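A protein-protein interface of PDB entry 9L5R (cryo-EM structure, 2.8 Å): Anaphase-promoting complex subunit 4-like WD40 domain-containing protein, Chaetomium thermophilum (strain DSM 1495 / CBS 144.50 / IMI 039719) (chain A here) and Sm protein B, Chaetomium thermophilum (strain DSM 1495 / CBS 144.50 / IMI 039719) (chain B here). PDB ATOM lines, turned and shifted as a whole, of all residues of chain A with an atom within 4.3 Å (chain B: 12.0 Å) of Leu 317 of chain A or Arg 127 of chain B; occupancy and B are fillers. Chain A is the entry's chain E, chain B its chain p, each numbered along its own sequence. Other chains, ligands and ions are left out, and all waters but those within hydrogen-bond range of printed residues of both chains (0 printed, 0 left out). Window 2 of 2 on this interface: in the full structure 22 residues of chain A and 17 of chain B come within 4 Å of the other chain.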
ATOM      1  N   LEU A  53      -4.681   1.623 -24.898  1.00  0.00           N
ATOM      2  CA  LEU A  53      -5.478   2.400 -23.961  1.00  0.00           C
ATOM      3  C   LEU A  53      -6.391   1.439 -23.224  1.00  0.00           C
ATOM      4  O   LEU A  53      -7.067   0.626 -23.860  1.00  0.00           O
ATOM      5  CB  LEU A  53      -6.302   3.468 -24.684  1.00  0.00           C
ATOM      6  CG  LEU A  53      -7.292   4.271 -23.848  1.00  0.00           C
ATOM      7  CD1 LEU A  53      -6.604   4.893 -22.666  1.00  0.00           C
ATOM      8  CD2 LEU A  53      -7.931   5.332 -24.700  1.00  0.00           C
ATOM      9  N   THR A 302     -10.734  16.352 -21.463  1.00  0.00           N
ATOM     10  CA  THR A 302      -9.518  16.185 -22.251  1.00  0.00           C
ATOM     11  C   THR A 302      -8.283  16.410 -21.400  1.00  0.00           C
ATOM     12  O   THR A 302      -8.179  17.420 -20.705  1.00  0.00           O
ATOM     13  CB  THR A 302      -9.487  17.141 -23.447  1.00  0.00           C
ATOM     14  OG1 THR A 302      -9.568  18.491 -22.983  1.00  0.00           O
ATOM     15  CG2 THR A 302     -10.623  16.859 -24.397  1.00  0.00           C
ATOM     16  N   VAL A 303      -7.341  15.483 -21.473  1.00  0.00           N
ATOM     17  CA  VAL A 303      -6.008  15.698 -20.930  1.00  0.00           C
ATOM     18  C   VAL A 303      -5.149  16.380 -21.989  1.00  0.00           C
ATOM     19  O   VAL A 303      -5.090  15.945 -23.146  1.00  0.00           O
ATOM     20  CB  VAL A 303      -5.394  14.377 -20.424  1.00  0.00           C
ATOM     21  CG1 VAL A 303      -5.377  13.310 -21.488  1.00  0.00           C
ATOM     22  CG2 VAL A 303      -3.986  14.608 -19.933  1.00  0.00           C
ATOM     23  N   TYR A 315      -0.379  17.188 -27.386  1.00  0.00           N
ATOM     24  CA  TYR A 315      -1.551  16.328 -27.458  1.00  0.00           C
ATOM     25  C   TYR A 315      -2.742  17.047 -26.850  1.00  0.00           C
ATOM     26  O   TYR A 315      -2.592  17.972 -26.052  1.00  0.00           O
ATOM     27  CB  TYR A 315      -1.348  15.006 -26.712  1.00  0.00           C
ATOM     28  CG  TYR A 315      -0.308  14.074 -27.279  1.00  0.00           C
ATOM     29  CD1 TYR A 315       1.033  14.221 -26.961  1.00  0.00           C
ATOM     30  CD2 TYR A 315      -0.672  13.022 -28.102  1.00  0.00           C
ATOM     31  CE1 TYR A 315       1.981  13.360 -27.464  1.00  0.00           C
ATOM     32  CE2 TYR A 315       0.269  12.154 -28.608  1.00  0.00           C
ATOM     33  CZ  TYR A 315       1.593  12.329 -28.286  1.00  0.00           C
ATOM     34  OH  TYR A 315       2.536  11.465 -28.791  1.00  0.00           O
ATOM     35  N   LYS A 316      -3.935  16.624 -27.257  1.00  0.00           N
ATOM     36  CA  LYS A 316      -5.191  17.038 -26.632  1.00  0.00           C
ATOM     37  C   LYS A 316      -6.107  15.828 -26.489  1.00  0.00           C
ATOM     38  O   LYS A 316      -7.234  15.815 -26.986  1.00  0.00           O
ATOM     39  CB  LYS A 316      -5.871  18.164 -27.399  1.00  0.00           C
ATOM     40  CG  LYS A 316      -6.841  18.965 -26.561  1.00  0.00           C
ATOM     41  CD  LYS A 316      -7.510  20.035 -27.374  1.00  0.00           C
ATOM     42  CE  LYS A 316      -8.929  20.252 -26.906  1.00  0.00           C
ATOM     43  NZ  LYS A 316      -8.980  20.728 -25.500  1.00  0.00           N
ATOM     44  N   LEU A 317      -5.589  14.776 -25.860  1.00  0.00           N
ATOM     45  CA  LEU A 317      -6.229  13.465 -25.841  1.00  0.00           C
ATOM     46  C   LEU A 317      -7.620  13.519 -25.206  1.00  0.00           C
ATOM     47  O   LEU A 317      -7.774  14.061 -24.106  1.00  0.00           O
ATOM     48  CB  LEU A 317      -5.344  12.503 -25.056  1.00  0.00           C
ATOM     49  CG  LEU A 317      -3.964  12.138 -25.600  1.00  0.00           C
ATOM     50  CD1 LEU A 317      -3.224  11.300 -24.590  1.00  0.00           C
ATOM     51  CD2 LEU A 317      -4.067  11.386 -26.896  1.00  0.00           C
ATOM     52  N   PRO A 318      -8.656  12.991 -25.873  1.00  0.00           N
ATOM     53  CA  PRO A 318     -10.000  12.961 -25.286  1.00  0.00           C
ATOM     54  C   PRO A 318     -10.220  11.742 -24.413  1.00  0.00           C
ATOM     55  O   PRO A 318      -9.268  11.037 -24.079  1.00  0.00           O
ATOM     56  CB  PRO A 318     -10.901  12.927 -26.518  1.00  0.00           C
ATOM     57  CG  PRO A 318     -10.114  12.115 -27.488  1.00  0.00           C
ATOM     58  CD  PRO A 318      -8.646  12.359 -27.199  1.00  0.00           C
ATOM     59  N   GLY A 319     -11.459  11.511 -23.991  1.00  0.00           N
ATOM     60  CA  GLY A 319     -11.794  10.220 -23.430  1.00  0.00           C
ATOM     61  C   GLY A 319     -12.686  10.224 -22.214  1.00  0.00           C
ATOM     62  O   GLY A 319     -13.121   9.164 -21.759  1.00  0.00           O
ATOM     63  N   ILE A 337       0.478   7.545 -19.925  1.00  0.00           N
ATOM     64  CA  ILE A 337      -0.253   8.646 -19.317  1.00  0.00           C
ATOM     65  C   ILE A 337      -1.501   8.080 -18.652  1.00  0.00           C
ATOM     66  O   ILE A 337      -2.110   7.127 -19.153  1.00  0.00           O
ATOM     67  CB  ILE A 337      -0.588   9.742 -20.357  1.00  0.00           C
ATOM     68  CG1 ILE A 337      -1.201  10.979 -19.700  1.00  0.00           C
ATOM     69  CG2 ILE A 337      -1.465   9.211 -21.471  1.00  0.00           C
ATOM     70  CD1 ILE A 337      -0.271  11.715 -18.800  1.00  0.00           C
ATOM     71  N   GLY A 349      -3.296   5.130 -20.957  1.00  0.00           N
ATOM     72  CA  GLY A 349      -2.885   4.956 -22.330  1.00  0.00           C
ATOM     73  C   GLY A 349      -1.381   5.104 -22.498  1.00  0.00           C
ATOM     74  O   GLY A 349      -0.660   5.480 -21.572  1.00  0.00           O
ATOM     75  N   LEU A 351       1.739   6.755 -25.122  1.00  0.00           N
ATOM     76  CA  LEU A 351       1.973   7.872 -26.032  1.00  0.00           C
ATOM     77  C   LEU A 351       2.857   7.394 -27.181  1.00  0.00           C
ATOM     78  O   LEU A 351       4.076   7.563 -27.188  1.00  0.00           O
ATOM     79  CB  LEU A 351       2.593   9.041 -25.279  1.00  0.00           C
ATOM     80  CG  LEU A 351       1.645   9.829 -24.376  1.00  0.00           C
ATOM     81  CD1 LEU A 351       2.276  11.141 -23.968  1.00  0.00           C
ATOM     82  CD2 LEU A 351       0.317  10.071 -25.063  1.00  0.00           C
ATOM     83  N   ARG B 123     -10.895  -2.901 -19.012  1.00  0.00           N
ATOM     84  CA  ARG B 123     -11.165  -3.303 -20.377  1.00  0.00           C
ATOM     85  C   ARG B 123     -10.459  -2.364 -21.341  1.00  0.00           C
ATOM     86  O   ARG B 123     -10.231  -1.193 -21.016  1.00  0.00           O
ATOM     87  CB  ARG B 123     -12.673  -3.304 -20.668  1.00  0.00           C
ATOM     88  CG  ARG B 123     -13.335  -1.960 -20.489  1.00  0.00           C
ATOM     89  CD  ARG B 123     -14.773  -2.004 -20.940  1.00  0.00           C
ATOM     90  NE  ARG B 123     -15.347  -0.671 -21.085  1.00  0.00           N
ATOM     91  CZ  ARG B 123     -15.219   0.083 -22.167  1.00  0.00           C
ATOM     92  NH1 ARG B 123     -14.512  -0.318 -23.210  1.00  0.00           N
ATOM     93  NH2 ARG B 123     -15.826   1.265 -22.209  1.00  0.00           N
ATOM     94  N   PRO B 124     -10.072  -2.857 -22.513  1.00  0.00           N
ATOM     95  CA  PRO B 124      -9.607  -1.957 -23.570  1.00  0.00           C
ATOM     96  C   PRO B 124     -10.729  -1.055 -24.051  1.00  0.00           C
ATOM     97  O   PRO B 124     -11.898  -1.441 -24.083  1.00  0.00           O
ATOM     98  CB  PRO B 124      -9.153  -2.912 -24.678  1.00  0.00           C
ATOM     99  CG  PRO B 124      -8.883  -4.190 -23.986  1.00  0.00           C
ATOM    100  CD  PRO B 124      -9.858  -4.270 -22.859  1.00  0.00           C
ATOM    101  N   ALA B 125     -10.361   0.162 -24.433  1.00  0.00           N
ATOM    102  CA  ALA B 125     -11.343   1.093 -24.960  1.00  0.00           C
ATOM    103  C   ALA B 125     -10.667   2.049 -25.925  1.00  0.00           C
ATOM    104  O   ALA B 125      -9.450   2.233 -25.901  1.00  0.00           O
ATOM    105  CB  ALA B 125     -12.039   1.879 -23.847  1.00  0.00           C
ATOM    106  N   GLY B 126     -11.483   2.651 -26.782  1.00  0.00           N
ATOM    107  CA  GLY B 126     -11.036   3.733 -27.625  1.00  0.00           C
ATOM    108  C   GLY B 126     -11.034   5.034 -26.867  1.00  0.00           C
ATOM    109  O   GLY B 126     -11.370   5.105 -25.688  1.00  0.00           O
ATOM    110  N   ARG B 127     -10.664   6.096 -27.567  1.00  0.00           N
ATOM    111  CA  ARG B 127     -10.413   7.364 -26.908  1.00  0.00           C
ATOM    112  C   ARG B 127     -11.393   8.467 -27.278  1.00  0.00           C
ATOM    113  O   ARG B 127     -11.629   9.351 -26.461  1.00  0.00           O
ATOM    114  CB  ARG B 127      -8.976   7.828 -27.197  1.00  0.00           C
ATOM    115  CG  ARG B 127      -8.461   8.853 -26.210  1.00  0.00           C
ATOM    116  CD  ARG B 127      -6.974   9.126 -26.315  1.00  0.00           C
ATOM    117  NE  ARG B 127      -6.171   8.331 -25.396  1.00  0.00           N
ATOM    118  CZ  ARG B 127      -5.951   8.651 -24.127  1.00  0.00           C
ATOM    119  NH1 ARG B 127      -6.516   9.709 -23.573  1.00  0.00           N
ATOM    120  NH2 ARG B 127      -5.141   7.890 -23.397  1.00  0.00           N
ATOM    121  N   GLY B 128     -11.980   8.451 -28.453  1.00  0.00           N
ATOM    122  CA  GLY B 128     -12.956   9.471 -28.782  1.00  0.00           C
ATOM    123  C   GLY B 128     -12.943   9.774 -30.263  1.00  0.00           C
ATOM    124  O   GLY B 128     -12.270   9.118 -31.050  1.00  0.00           O
ATOM    125  N   ALA B 129     -13.731  10.784 -30.632  1.00  0.00           N
ATOM    126  CA  ALA B 129     -13.827  11.133 -32.045  1.00  0.00           C
ATOM    127  C   ALA B 129     -12.700  12.068 -32.475  1.00  0.00           C
ATOM    128  O   ALA B 129     -11.805  11.671 -33.225  1.00  0.00           O
ATOM    129  CB  ALA B 129     -15.193  11.759 -32.339  1.00  0.00           C
ATOM    130  N   ALA B 130     -12.720  13.306 -32.001  1.00  0.00           N
ATOM    131  CA  ALA B 130     -11.715  14.230 -32.516  1.00  0.00           C
ATOM    132  C   ALA B 130     -11.018  15.056 -31.452  1.00  0.00           C
ATOM    133  O   ALA B 130      -9.798  15.215 -31.522  1.00  0.00           O
ATOM    134  CB  ALA B 130     -12.360  15.169 -33.548  1.00  0.00           C
ATOM    135  N   ALA B 131     -11.758  15.553 -30.454  1.00  0.00           N
ATOM    136  CA  ALA B 131     -11.339  16.591 -29.512  1.00  0.00           C
ATOM    137  C   ALA B 131     -10.732  17.790 -30.239  1.00  0.00           C
ATOM    138  O   ALA B 131      -9.508  17.967 -30.219  1.00  0.00           O
ATOM    139  CB  ALA B 131     -10.351  16.041 -28.478  1.00  0.00           C
ATOM    140  N   PRO B 132     -11.536  18.612 -30.917  1.00  0.00           N
ATOM    141  CA  PRO B 132     -10.983  19.795 -31.581  1.00  0.00           C
ATOM    142  C   PRO B 132     -10.496  20.836 -30.584  1.00  0.00           C
ATOM    143  O   PRO B 132     -11.014  20.961 -29.472  1.00  0.00           O
ATOM    144  CB  PRO B 132     -12.163  20.327 -32.397  1.00  0.00           C
ATOM    145  CG  PRO B 132     -13.355  19.872 -31.648  1.00  0.00           C
ATOM    146  CD  PRO B 132     -12.997  18.528 -31.084  1.00  0.00           C
ATOM    147  N   ILE B 133      -9.489  21.595 -31.007  1.00  0.00           N
ATOM    148  CA  ILE B 133      -8.886  22.630 -30.174  1.00  0.00           C
ATOM    149  C   ILE B 133      -9.796  23.848 -30.074  1.00  0.00           C
ATOM    150  O   ILE B 133      -9.970  24.586 -31.042  1.00  0.00           O
ATOM    151  CB  ILE B 133      -7.505  23.032 -30.712  1.00  0.00           C
ATOM    152  CG1 ILE B 133      -6.582  21.814 -30.766  1.00  0.00           C
ATOM    153  CG2 ILE B 133      -6.902  24.126 -29.858  1.00  0.00           C
ATOM    154  CD1 ILE B 133      -5.283  22.065 -31.486  1.00  0.00           C
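The backbone NH (N) of Ala 125 of chain B lies within hydrogen-bond range of the backbone carbonyl oxygen (O) of Leu 53 of chain A.
The backbone carbonyl oxygen (O) of Pro 318 of chain A sits at hydrogen-bond distance from the guanidinium group (NH1) of Arg 127 of chain B (3.1 Å).
O of Arg 127 of chain B lies close to N of Gly 319 of chain A (3.3 Å).
The side-chain hydroxyl of Thr 302 of chain A lies within hydrogen-bond range of the side-chain amino group of Lys 316 of chain A (3.4 Å).
O of Val 303 of chain A is in hydrogen-bond range of N of Leu 317 of chain A (3.0 Å).
The backbone carbonyl oxygen (O) of Gly 349 of chain A is in hydrogen-bond range of the backbone NH (N) of Ile 337 of chain A, at 2.9 Å.
Leu 53 of chain A touches Pro 124 of chain B (O to CA, 3.6 Å).
Gly 126 of chain B touches Leu 53 of chain A (O to CD2, 3.6 Å).
Leu 53 of chain A touches Arg 127 of chain B.
CB of Ala 131 of chain B touches O of Lys 316 of chain A (3.5 Å).
Pro 132 of chain B touches Lys 316 of chain A.
Lys 316 of chain A touches Ile 133 of chain B (CD to CG1, 3.9 Å).
Leu 317 of chain A touches Arg 127 of chain B (CB to NH1, 3.4 Å).
CB of Pro 318 of chain A touches CB of Ala 131 of chain B, 3.7 Å away.
Arg 127 of chain B touches Gly 349 of chain A.
No residue of chain B comes within 4 Å of Thr 302 of chain A.
Printed residues of chain B within 4 Å of Lys 316 of chain A: Ala 131 (3.5 Å), Pro 132 (3.4 Å) and Ile 133 (3.9 Å).
Leu 317 of chain A touches one residue of chain B.
Of chain B, only Arg 127 (3.1 Å) and Ala 131 (3.7 Å) come within 4 Å of Pro 318 of chain A.
Of the printed residues of chain B, Gly 319 of chain A touches Arg 127 (3.2 Å).
Printed residues of chain B within 4 Å of Gly 349 of chain A: Arg 127.
Leu 351 of chain A touches none of the printed residues of chain B.
Printed residues of chain A within 4 Å of Ala 125 of chain B: Leu 53 (3.4 Å).
Of the printed residues of chain A, Gly 126 of chain B touches Leu 53.
Arg 127 of chain B touches just these residues of chain A: Leu 53 (3.4 Å), Leu 317 (3.4 Å), Pro 318 (3.1 Å), Gly 319 (3.2 Å) and Gly 349 (3.9 Å).
Ala 130 of chain B touches none of the printed residues of chain A.
Of the printed residues of chain A, Ala 131 of chain B touches Lys 316 and Pro 318.
The nearest residue of chain B that does not touch Leu 317 of chain A is Ala 131 of chain B (5.0 Å).
The nearest printed residue of chain A that does not touch Arg 127 of chain B is Val 303 of chain A (4.3 Å).
The nearest printed residue of chain A that does not touch Gly 126 of chain B is Gly 319 of chain A (5.6 Å).
Hydrophobic or aromatic side chains of chain B within 4 Å of the printed part of chain A: Ala 131 and Ile 133.
Of the 11 printed residues of chain A, 6 touch a printed residue of chain B.
Hydrophobic or aromatic side chains of chain A within 4 Å of the printed part of chain B: Leu 53, Leu 317 and Pro 318.
Along chain A the printed residues that touch a printed residue of chain B span positions 53 to 349.
Among the printed residues, 12 pairs touch across the chains.
Among the printed residues, no Asp or Glu carboxylate lies within 4 Å of a Lys or Arg side-chain nitrogen of the other chain.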
